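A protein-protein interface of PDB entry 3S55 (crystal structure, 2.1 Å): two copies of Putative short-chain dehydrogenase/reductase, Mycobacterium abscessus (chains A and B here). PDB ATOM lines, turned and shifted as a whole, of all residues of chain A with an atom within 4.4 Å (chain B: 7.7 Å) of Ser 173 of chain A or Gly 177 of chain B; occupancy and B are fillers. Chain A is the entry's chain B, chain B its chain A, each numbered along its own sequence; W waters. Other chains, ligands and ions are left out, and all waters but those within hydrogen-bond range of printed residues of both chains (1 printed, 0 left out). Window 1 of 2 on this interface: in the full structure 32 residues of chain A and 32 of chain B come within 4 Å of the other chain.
Leu 131 of chain B touches Trp 123 of chain A (CG to CZ2, 3.9 Å).
Phe 135 of chain B touches Trp 123 of chain A (CD1 to CE3, 3.5 Å).
Ala 169 of chain A touches Cys 184 of chain B.
Val 172 of chain A touches Gly 180 of chain B.
Val 172 of chain A touches Cys 184 of chain B (CB to SG, 3.4 Å).
CA of Gly 177 of chain B touches O of Ser 173 of chain A (3.5 Å).
CB of Leu 181 of chain B touches OG of Ser 173 of chain A (3.3 Å).
O of Trp 176 of chain B touches CB of Trp 176 of chain A, 3.4 Å away.
Trp 176 of chain A touches Ile 179 of chain B.
Trp 176 of chain A touches Gly 180 of chain B (CG to CA, 3.5 Å).
OG1 of Thr 132 of chain B sits at hydrogen-bond distance from NE1 of Trp 123 of chain A.
Water W1 bridges the backbone NH of Ala 169 of chain A (3.4 Å) and the backbone carbonyl oxygen of Cys 184 of chain B (3.5 Å).
The backbone carbonyl oxygen (O) of Gly 161 of chain B lies close to the indole nitrogen (NE1) of Trp 176 of chain B, at 3.3 Å.
The backbone carbonyl oxygen (O) of Gly 180 of chain B sits at hydrogen-bond distance from the side-chain sulfur (SG) of Cys 184 of chain B (3.4 Å).
OG of Ser 173 of chain A lies within hydrogen-bond range of O of Ala 169 of chain A (2.7 Å).
Of chain B, only Gly 177 (3.5 Å) and Leu 181 (3.3 Å) come within 4 Å of Ser 173 of chain A.
Of the printed residues of chain A, Phe 135 of chain B touches Trp 123.
Of the printed residues of chain A, Ser 173 of chain B touches Gly 177 (3.6 Å).
Of chain A, only Ser 173 comes within 4 Å of Gly 177 of chain B.
Of the printed residues of chain A, Ile 179 of chain B touches Trp 176 (3.4 Å).
Of the printed residues of chain A, Leu 181 of chain B touches Ser 173.
Thr 182 of chain B touches none of the printed residues of chain A.
The nearest residue of chain A that does not touch Gly 177 of chain B is Gly 177 of chain A (4.02 Å).
Ser 173 of chain A touches Gly 177 of chain B, and with the chains exchanged Gly 177 of chain A touches Ser 173 of chain B.
Trp 176 of chain A touches its own counterpart, Trp 176 of chain B.
7 positions are printed for both chains.
Of the 13 pairs that touch across the chains among the printed residues, 3 have their exchanged pair printed and touching as well.
Hydrophobic or aromatic side chains of chain A within 4 Å of the printed part of chain B: Trp 123, Val 172 and Trp 176.
Hydrophobic or aromatic side chains of chain B that line the printed part of chain A: Leu 131, Phe 135, Trp 176, Ile 179 and Leu 181.
Among the printed residues, 13 pairs touch across the chains.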
ATOM      1  N   TRP A 123     -23.078 -30.096  13.392  1.00  0.00           N
ATOM      2  CA  TRP A 123     -22.526 -29.832  12.058  1.00  0.00           C
ATOM      3  C   TRP A 123     -21.009 -30.072  12.042  1.00  0.00           C
ATOM      4  O   TRP A 123     -20.512 -30.824  11.194  1.00  0.00           O
ATOM      5  CB  TRP A 123     -22.853 -28.401  11.614  1.00  0.00           C
ATOM      6  CG  TRP A 123     -22.205 -27.990  10.328  1.00  0.00           C
ATOM      7  CD1 TRP A 123     -21.003 -27.361  10.187  1.00  0.00           C
ATOM      8  CD2 TRP A 123     -22.722 -28.171   8.995  1.00  0.00           C
ATOM      9  NE1 TRP A 123     -20.733 -27.139   8.857  1.00  0.00           N
ATOM     10  CE2 TRP A 123     -21.780 -27.610   8.103  1.00  0.00           C
ATOM     11  CE3 TRP A 123     -23.890 -28.733   8.474  1.00  0.00           C
ATOM     12  CZ2 TRP A 123     -21.967 -27.606   6.722  1.00  0.00           C
ATOM     13  CZ3 TRP A 123     -24.083 -28.714   7.096  1.00  0.00           C
ATOM     14  CH2 TRP A 123     -23.129 -28.165   6.237  1.00  0.00           C
ATOM     15  N   ILE A 127     -19.520 -33.017   9.559  1.00  0.00           N
ATOM     16  CA  ILE A 127     -18.529 -32.544   8.592  1.00  0.00           C
ATOM     17  C   ILE A 127     -17.132 -33.047   8.993  1.00  0.00           C
ATOM     18  O   ILE A 127     -16.324 -33.485   8.142  1.00  0.00           O
ATOM     19  CB  ILE A 127     -18.541 -30.972   8.475  1.00  0.00           C
ATOM     20  CG1 ILE A 127     -19.883 -30.441   7.943  1.00  0.00           C
ATOM     21  CG2 ILE A 127     -17.407 -30.474   7.574  1.00  0.00           C
ATOM     22  CD1 ILE A 127     -20.426 -31.140   6.673  1.00  0.00           C
ATOM     23  N   ALA A 169     -29.091 -31.980   6.447  1.00  0.00           N
ATOM     24  CA  ALA A 169     -28.091 -31.030   5.960  1.00  0.00           C
ATOM     25  C   ALA A 169     -26.635 -31.394   6.270  1.00  0.00           C
ATOM     26  O   ALA A 169     -25.826 -31.441   5.363  1.00  0.00           O
ATOM     27  CB  ALA A 169     -28.409 -29.638   6.433  1.00  0.00           C
ATOM     28  N   SER A 170     -26.293 -31.649   7.530  1.00  0.00           N
ATOM     29  CA  SER A 170     -24.910 -32.037   7.892  1.00  0.00           C
ATOM     30  C   SER A 170     -24.416 -33.275   7.147  1.00  0.00           C
ATOM     31  O   SER A 170     -23.335 -33.243   6.547  1.00  0.00           O
ATOM     32  CB  SER A 170     -24.741 -32.250   9.396  1.00  0.00           C
ATOM     33  OG  SER A 170     -25.252 -31.145  10.132  1.00  0.00           O
ATOM     34  N   TYR A 171     -25.200 -34.358   7.215  1.00  0.00           N
ATOM     35  CA  TYR A 171     -24.816 -35.663   6.625  1.00  0.00           C
ATOM     36  C   TYR A 171     -24.699 -35.606   5.097  1.00  0.00           C
ATOM     37  O   TYR A 171     -23.733 -36.061   4.502  1.00  0.00           O
ATOM     38  CB  TYR A 171     -25.818 -36.762   7.042  1.00  0.00           C
ATOM     39  CG  TYR A 171     -25.424 -38.169   6.600  1.00  0.00           C
ATOM     40  CD1 TYR A 171     -24.480 -38.906   7.328  1.00  0.00           C
ATOM     41  CD2 TYR A 171     -25.999 -38.773   5.475  1.00  0.00           C
ATOM     42  CE1 TYR A 171     -24.097 -40.180   6.959  1.00  0.00           C
ATOM     43  CE2 TYR A 171     -25.612 -40.105   5.086  1.00  0.00           C
ATOM     44  CZ  TYR A 171     -24.658 -40.786   5.850  1.00  0.00           C
ATOM     45  OH  TYR A 171     -24.213 -42.059   5.520  1.00  0.00           O
ATOM     46  N   VAL A 172     -25.705 -35.028   4.472  1.00  0.00           N
ATOM     47  CA  VAL A 172     -25.738 -34.900   3.021  1.00  0.00           C
ATOM     48  C   VAL A 172     -24.612 -33.987   2.487  1.00  0.00           C
ATOM     49  O   VAL A 172     -23.951 -34.339   1.508  1.00  0.00           O
ATOM     50  CB  VAL A 172     -27.126 -34.446   2.571  1.00  0.00           C
ATOM     51  CG1 VAL A 172     -27.144 -34.125   1.077  1.00  0.00           C
ATOM     52  CG2 VAL A 172     -28.162 -35.543   2.911  1.00  0.00           C
ATOM     53  N   SER A 173     -24.388 -32.839   3.139  1.00  0.00           N
ATOM     54  CA  SER A 173     -23.287 -31.931   2.747  1.00  0.00           C
ATOM     55  C   SER A 173     -21.951 -32.669   2.847  1.00  0.00           C
ATOM     56  O   SER A 173     -21.094 -32.548   1.987  1.00  0.00           O
ATOM     57  CB  SER A 173     -23.230 -30.692   3.650  1.00  0.00           C
ATOM     58  OG  SER A 173     -24.420 -29.937   3.595  1.00  0.00           O
ATOM     59  N   SER A 174     -21.785 -33.450   3.904  1.00  0.00           N
ATOM     60  CA  SER A 174     -20.560 -34.245   4.052  1.00  0.00           C
ATOM     61  C   SER A 174     -20.384 -35.298   2.930  1.00  0.00           C
ATOM     62  O   SER A 174     -19.295 -35.413   2.361  1.00  0.00           O
ATOM     63  CB  SER A 174     -20.487 -34.841   5.464  1.00  0.00           C
ATOM     64  OG  SER A 174     -21.340 -35.961   5.635  1.00  0.00           O
ATOM     65  N   LYS A 175     -21.445 -36.033   2.589  1.00  0.00           N
ATOM     66  CA  LYS A 175     -21.344 -37.116   1.596  1.00  0.00           C
ATOM     67  C   LYS A 175     -21.176 -36.629   0.125  1.00  0.00           C
ATOM     68  O   LYS A 175     -20.557 -37.340  -0.688  1.00  0.00           O
ATOM     69  CB  LYS A 175     -22.502 -38.128   1.700  1.00  0.00           C
ATOM     70  CG  LYS A 175     -22.598 -38.873   3.056  1.00  0.00           C
ATOM     71  CD  LYS A 175     -21.277 -39.601   3.392  1.00  0.00           C
ATOM     72  CE  LYS A 175     -21.477 -40.619   4.516  1.00  0.00           C
ATOM     73  NZ  LYS A 175     -20.292 -41.552   4.626  1.00  0.00           N
ATOM     74  N   TRP A 176     -21.745 -35.457  -0.173  1.00  0.00           N
ATOM     75  CA  TRP A 176     -21.464 -34.702  -1.392  1.00  0.00           C
ATOM     76  C   TRP A 176     -20.001 -34.293  -1.412  1.00  0.00           C
ATOM     77  O   TRP A 176     -19.323 -34.520  -2.415  1.00  0.00           O
ATOM     78  CB  TRP A 176     -22.375 -33.467  -1.523  1.00  0.00           C
ATOM     79  CG  TRP A 176     -23.732 -33.834  -2.083  1.00  0.00           C
ATOM     80  CD1 TRP A 176     -24.724 -34.527  -1.457  1.00  0.00           C
ATOM     81  CD2 TRP A 176     -24.225 -33.516  -3.392  1.00  0.00           C
ATOM     82  NE1 TRP A 176     -25.812 -34.659  -2.291  1.00  0.00           N
ATOM     83  CE2 TRP A 176     -25.532 -34.046  -3.486  1.00  0.00           C
ATOM     84  CE3 TRP A 176     -23.683 -32.822  -4.494  1.00  0.00           C
ATOM     85  CZ2 TRP A 176     -26.312 -33.927  -4.648  1.00  0.00           C
ATOM     86  CZ3 TRP A 176     -24.455 -32.701  -5.668  1.00  0.00           C
ATOM     87  CH2 TRP A 176     -25.758 -33.256  -5.727  1.00  0.00           C
ATOM     88  N   GLY A 177     -19.529 -33.704  -0.309  1.00  0.00           N
ATOM     89  CA  GLY A 177     -18.115 -33.349  -0.149  1.00  0.00           C
ATOM     90  C   GLY A 177     -17.168 -34.503  -0.449  1.00  0.00           C
ATOM     91  O   GLY A 177     -16.144 -34.317  -1.109  1.00  0.00           O
ATOM     92  N   ASN B 130     -16.207 -21.529   3.016  1.00  0.00           N
ATOM     93  CA  ASN B 130     -17.042 -21.840   1.838  1.00  0.00           C
ATOM     94  C   ASN B 130     -18.256 -22.723   2.134  1.00  0.00           C
ATOM     95  O   ASN B 130     -19.309 -22.519   1.564  1.00  0.00           O
ATOM     96  CB  ASN B 130     -16.208 -22.528   0.737  1.00  0.00           C
ATOM     97  CG  ASN B 130     -15.170 -21.610   0.104  1.00  0.00           C
ATOM     98  OD1 ASN B 130     -15.056 -20.438   0.451  1.00  0.00           O
ATOM     99  ND2 ASN B 130     -14.417 -22.146  -0.859  1.00  0.00           N
ATOM    100  N   LEU B 131     -18.103 -23.725   2.999  1.00  0.00           N
ATOM    101  CA  LEU B 131     -19.193 -24.685   3.211  1.00  0.00           C
ATOM    102  C   LEU B 131     -19.936 -24.423   4.538  1.00  0.00           C
ATOM    103  O   LEU B 131     -21.138 -24.150   4.528  1.00  0.00           O
ATOM    104  CB  LEU B 131     -18.656 -26.124   3.130  1.00  0.00           C
ATOM    105  CG  LEU B 131     -19.567 -27.254   3.624  1.00  0.00           C
ATOM    106  CD1 LEU B 131     -20.936 -27.274   2.899  1.00  0.00           C
ATOM    107  CD2 LEU B 131     -18.802 -28.566   3.389  1.00  0.00           C
ATOM    108  N   THR B 132     -19.219 -24.493   5.669  1.00  0.00           N
ATOM    109  CA  THR B 132     -19.797 -24.125   6.971  1.00  0.00           C
ATOM    110  C   THR B 132     -20.341 -22.669   6.982  1.00  0.00           C
ATOM    111  O   THR B 132     -21.378 -22.403   7.560  1.00  0.00           O
ATOM    112  CB  THR B 132     -18.766 -24.345   8.122  1.00  0.00           C
ATOM    113  OG1 THR B 132     -18.257 -25.678   8.050  1.00  0.00           O
ATOM    114  CG2 THR B 132     -19.377 -24.092   9.530  1.00  0.00           C
ATOM    115  N   THR B 134     -21.636 -21.039   4.519  1.00  0.00           N
ATOM    116  CA  THR B 134     -22.917 -21.143   3.806  1.00  0.00           C
ATOM    117  C   THR B 134     -23.986 -21.710   4.721  1.00  0.00           C
ATOM    118  O   THR B 134     -25.103 -21.168   4.795  1.00  0.00           O
ATOM    119  CB  THR B 134     -22.770 -22.014   2.547  1.00  0.00           C
ATOM    120  OG1 THR B 134     -21.904 -21.331   1.617  1.00  0.00           O
ATOM    121  CG2 THR B 134     -24.152 -22.264   1.884  1.00  0.00           C
ATOM    122  N   PHE B 135     -23.644 -22.806   5.406  1.00  0.00           N
ATOM    123  CA  PHE B 135     -24.523 -23.378   6.420  1.00  0.00           C
ATOM    124  C   PHE B 135     -24.918 -22.309   7.445  1.00  0.00           C
ATOM    125  O   PHE B 135     -26.093 -22.157   7.741  1.00  0.00           O
ATOM    126  CB  PHE B 135     -23.860 -24.571   7.120  1.00  0.00           C
ATOM    127  CG  PHE B 135     -24.513 -24.946   8.433  1.00  0.00           C
ATOM    128  CD1 PHE B 135     -25.660 -25.738   8.456  1.00  0.00           C
ATOM    129  CD2 PHE B 135     -23.977 -24.502   9.645  1.00  0.00           C
ATOM    130  CE1 PHE B 135     -26.256 -26.077   9.662  1.00  0.00           C
ATOM    131  CE2 PHE B 135     -24.578 -24.820  10.865  1.00  0.00           C
ATOM    132  CZ  PHE B 135     -25.703 -25.617  10.877  1.00  0.00           C
ATOM    133  N   SER B 157     -21.741 -21.995  -5.675  1.00  0.00           N
ATOM    134  CA  SER B 157     -20.872 -23.130  -5.795  1.00  0.00           C
ATOM    135  C   SER B 157     -19.846 -22.756  -6.835  1.00  0.00           C
ATOM    136  O   SER B 157     -19.290 -21.658  -6.794  1.00  0.00           O
ATOM    137  CB  SER B 157     -21.661 -24.392  -6.166  1.00  0.00           C
ATOM    138  OG  SER B 157     -20.784 -25.494  -6.411  1.00  0.00           O
ATOM    139  N   GLY B 161     -17.810 -27.343  -8.497  1.00  0.00           N
ATOM    140  CA  GLY B 161     -18.794 -27.991  -7.607  1.00  0.00           C
ATOM    141  C   GLY B 161     -19.448 -29.238  -8.204  1.00  0.00           C
ATOM    142  O   GLY B 161     -20.111 -29.975  -7.504  1.00  0.00           O
ATOM    143  N   TYR B 171     -10.941 -26.611  -2.019  1.00  0.00           N
ATOM    144  CA  TYR B 171     -11.931 -25.830  -2.731  1.00  0.00           C
ATOM    145  C   TYR B 171     -13.066 -26.707  -3.308  1.00  0.00           C
ATOM    146  O   TYR B 171     -14.232 -26.456  -3.004  1.00  0.00           O
ATOM    147  CB  TYR B 171     -11.252 -25.022  -3.823  1.00  0.00           C
ATOM    148  CG  TYR B 171     -12.152 -24.023  -4.474  1.00  0.00           C
ATOM    149  CD1 TYR B 171     -12.462 -22.820  -3.833  1.00  0.00           C
ATOM    150  CD2 TYR B 171     -12.689 -24.261  -5.728  1.00  0.00           C
ATOM    151  CE1 TYR B 171     -13.274 -21.870  -4.431  1.00  0.00           C
ATOM    152  CE2 TYR B 171     -13.502 -23.319  -6.336  1.00  0.00           C
ATOM    153  CZ  TYR B 171     -13.796 -22.128  -5.673  1.00  0.00           C
ATOM    154  OH  TYR B 171     -14.602 -21.181  -6.278  1.00  0.00           O
ATOM    155  N   VAL B 172     -12.720 -27.724  -4.108  1.00  0.00           N
ATOM    156  CA  VAL B 172     -13.723 -28.660  -4.714  1.00  0.00           C
ATOM    157  C   VAL B 172     -14.616 -29.407  -3.698  1.00  0.00           C
ATOM    158  O   VAL B 172     -15.835 -29.493  -3.875  1.00  0.00           O
ATOM    159  CB  VAL B 172     -13.083 -29.686  -5.705  1.00  0.00           C
ATOM    160  CG1 VAL B 172     -14.134 -30.652  -6.311  1.00  0.00           C
ATOM    161  CG2 VAL B 172     -12.407 -28.976  -6.810  1.00  0.00           C
ATOM    162  N   SER B 173     -14.029 -29.949  -2.645  1.00  0.00           N
ATOM    163  CA  SER B 173     -14.854 -30.556  -1.569  1.00  0.00           C
ATOM    164  C   SER B 173     -15.898 -29.599  -1.001  1.00  0.00           C
ATOM    165  O   SER B 173     -17.034 -30.006  -0.743  1.00  0.00           O
ATOM    166  CB  SER B 173     -13.990 -31.064  -0.414  1.00  0.00           C
ATOM    167  OG  SER B 173     -13.019 -31.943  -0.902  1.00  0.00           O
ATOM    168  N   SER B 174     -15.504 -28.350  -0.762  1.00  0.00           N
ATOM    169  CA  SER B 174     -16.447 -27.394  -0.216  1.00  0.00           C
ATOM    170  C   SER B 174     -17.579 -27.050  -1.202  1.00  0.00           C
ATOM    171  O   SER B 174     -18.724 -26.880  -0.780  1.00  0.00           O
ATOM    172  CB  SER B 174     -15.757 -26.130   0.330  1.00  0.00           C
ATOM    173  OG  SER B 174     -15.259 -25.303  -0.714  1.00  0.00           O
ATOM    174  N   LYS B 175     -17.253 -26.935  -2.488  1.00  0.00           N
ATOM    175  CA  LYS B 175     -18.231 -26.519  -3.500  1.00  0.00           C
ATOM    176  C   LYS B 175     -19.181 -27.670  -3.913  1.00  0.00           C
ATOM    177  O   LYS B 175     -20.325 -27.414  -4.335  1.00  0.00           O
ATOM    178  CB  LYS B 175     -17.530 -25.881  -4.713  1.00  0.00           C
ATOM    179  CG  LYS B 175     -16.716 -24.580  -4.395  1.00  0.00           C
ATOM    180  CD  LYS B 175     -17.629 -23.441  -3.884  1.00  0.00           C
ATOM    181  CE  LYS B 175     -16.948 -22.100  -3.880  1.00  0.00           C
ATOM    182  NZ  LYS B 175     -17.915 -21.011  -3.472  1.00  0.00           N
ATOM    183  N   TRP B 176     -18.722 -28.918  -3.756  1.00  0.00           N
ATOM    184  CA  TRP B 176     -19.614 -30.088  -3.862  1.00  0.00           C
ATOM    185  C   TRP B 176     -20.552 -30.138  -2.679  1.00  0.00           C
ATOM    186  O   TRP B 176     -21.713 -30.373  -2.852  1.00  0.00           O
ATOM    187  CB  TRP B 176     -18.824 -31.406  -3.948  1.00  0.00           C
ATOM    188  CG  TRP B 176     -18.377 -31.756  -5.376  1.00  0.00           C
ATOM    189  CD1 TRP B 176     -17.400 -31.120  -6.110  1.00  0.00           C
ATOM    190  CD2 TRP B 176     -18.879 -32.820  -6.216  1.00  0.00           C
ATOM    191  NE1 TRP B 176     -17.282 -31.715  -7.355  1.00  0.00           N
ATOM    192  CE2 TRP B 176     -18.168 -32.765  -7.437  1.00  0.00           C
ATOM    193  CE3 TRP B 176     -19.859 -33.806  -6.055  1.00  0.00           C
ATOM    194  CZ2 TRP B 176     -18.418 -33.670  -8.506  1.00  0.00           C
ATOM    195  CZ3 TRP B 176     -20.104 -34.712  -7.115  1.00  0.00           C
ATOM    196  CH2 TRP B 176     -19.379 -34.631  -8.318  1.00  0.00           C
ATOM    197  N   GLY B 177     -20.037 -29.888  -1.471  1.00  0.00           N
ATOM    198  CA  GLY B 177     -20.876 -29.895  -0.259  1.00  0.00           C
ATOM    199  C   GLY B 177     -21.940 -28.796  -0.272  1.00  0.00           C
ATOM    200  O   GLY B 177     -23.058 -29.008   0.188  1.00  0.00           O
ATOM    201  N   VAL B 178     -21.579 -27.628  -0.814  1.00  0.00           N
ATOM    202  CA  VAL B 178     -22.515 -26.509  -1.009  1.00  0.00           C
ATOM    203  C   VAL B 178     -23.770 -26.925  -1.822  1.00  0.00           C
ATOM    204  O   VAL B 178     -24.899 -26.517  -1.496  1.00  0.00           O
ATOM    205  CB  VAL B 178     -21.854 -25.285  -1.746  1.00  0.00           C
ATOM    206  CG1 VAL B 178     -22.926 -24.273  -2.196  1.00  0.00           C
ATOM    207  CG2 VAL B 178     -20.860 -24.558  -0.821  1.00  0.00           C
ATOM    208  N   ILE B 179     -23.543 -27.670  -2.907  1.00  0.00           N
ATOM    209  CA  ILE B 179     -24.637 -28.196  -3.703  1.00  0.00           C
ATOM    210  C   ILE B 179     -25.491 -29.163  -2.874  1.00  0.00           C
ATOM    211  O   ILE B 179     -26.719 -29.033  -2.845  1.00  0.00           O
ATOM    212  CB  ILE B 179     -24.159 -28.836  -5.042  1.00  0.00           C
ATOM    213  CG1 ILE B 179     -23.500 -27.764  -5.929  1.00  0.00           C
ATOM    214  CG2 ILE B 179     -25.357 -29.465  -5.802  1.00  0.00           C
ATOM    215  CD1 ILE B 179     -23.036 -28.248  -7.263  1.00  0.00           C
ATOM    216  N   GLY B 180     -24.861 -30.113  -2.176  1.00  0.00           N
ATOM    217  CA  GLY B 180     -25.627 -30.983  -1.262  1.00  0.00           C
ATOM    218  C   GLY B 180     -26.443 -30.177  -0.246  1.00  0.00           C
ATOM    219  O   GLY B 180     -27.655 -30.443  -0.024  1.00  0.00           O
ATOM    220  N   LEU B 181     -25.766 -29.224   0.407  1.00  0.00           N
ATOM    221  CA  LEU B 181     -26.389 -28.284   1.353  1.00  0.00           C
ATOM    222  C   LEU B 181     -27.568 -27.516   0.735  1.00  0.00           C
ATOM    223  O   LEU B 181     -28.600 -27.340   1.366  1.00  0.00           O
ATOM    224  CB  LEU B 181     -25.342 -27.276   1.879  1.00  0.00           C
ATOM    225  CG  LEU B 181     -25.738 -26.200   2.906  1.00  0.00           C
ATOM    226  CD1 LEU B 181     -26.346 -26.862   4.115  1.00  0.00           C
ATOM    227  CD2 LEU B 181     -24.524 -25.369   3.306  1.00  0.00           C
ATOM    228  N   THR B 182     -27.384 -27.036  -0.482  1.00  0.00           N
ATOM    229  CA  THR B 182     -28.431 -26.296  -1.220  1.00  0.00           C
ATOM    230  C   THR B 182     -29.704 -27.137  -1.319  1.00  0.00           C
ATOM    231  O   THR B 182     -30.799 -26.667  -0.985  1.00  0.00           O
ATOM    232  CB  THR B 182     -27.881 -25.851  -2.597  1.00  0.00           C
ATOM    233  OG1 THR B 182     -26.854 -24.872  -2.362  1.00  0.00           O
ATOM    234  CG2 THR B 182     -28.991 -25.198  -3.476  1.00  0.00           C
ATOM    235  N   LYS B 183     -29.545 -28.421  -1.657  1.00  0.00           N
ATOM    236  CA  LYS B 183     -30.699 -29.265  -1.871  1.00  0.00           C
ATOM    237  C   LYS B 183     -31.436 -29.651  -0.549  1.00  0.00           C
ATOM    238  O   LYS B 183     -32.668 -29.814  -0.531  1.00  0.00           O
ATOM    239  CB  LYS B 183     -30.301 -30.494  -2.709  1.00  0.00           C
ATOM    240  CG  LYS B 183     -29.834 -30.136  -4.121  1.00  0.00           C
ATOM    241  CD  LYS B 183     -29.332 -31.381  -4.888  1.00  0.00           C
ATOM    242  CE  LYS B 183     -28.842 -31.034  -6.302  1.00  0.00           C
ATOM    243  NZ  LYS B 183     -29.964 -30.691  -7.244  1.00  0.00           N
ATOM    244  N   CYS B 184     -30.674 -29.776   0.536  1.00  0.00           N
ATOM    245  CA  CYS B 184     -31.233 -30.003   1.894  1.00  0.00           C
ATOM    246  C   CYS B 184     -32.005 -28.805   2.448  1.00  0.00           C
ATOM    247  O   CYS B 184     -33.128 -28.935   2.990  1.00  0.00           O
ATOM    248  CB  CYS B 184     -30.102 -30.339   2.858  1.00  0.00           C
ATOM    249  SG  CYS B 184     -29.366 -31.931   2.504  1.00  0.00           S
ATOM    250  N   ALA B 185     -31.394 -27.633   2.328  1.00  0.00           N
ATOM    251  CA  ALA B 185     -32.072 -26.414   2.753  1.00  0.00           C
ATOM    252  C   ALA B 185     -33.377 -26.266   1.971  1.00  0.00           C
ATOM    253  O   ALA B 185     -34.418 -25.898   2.538  1.00  0.00           O
ATOM    254  CB  ALA B 185     -31.179 -25.233   2.559  1.00  0.00           C
HETATM  255  O   HOH W   1     -32.115 -31.686   4.819  1.00  0.00           O
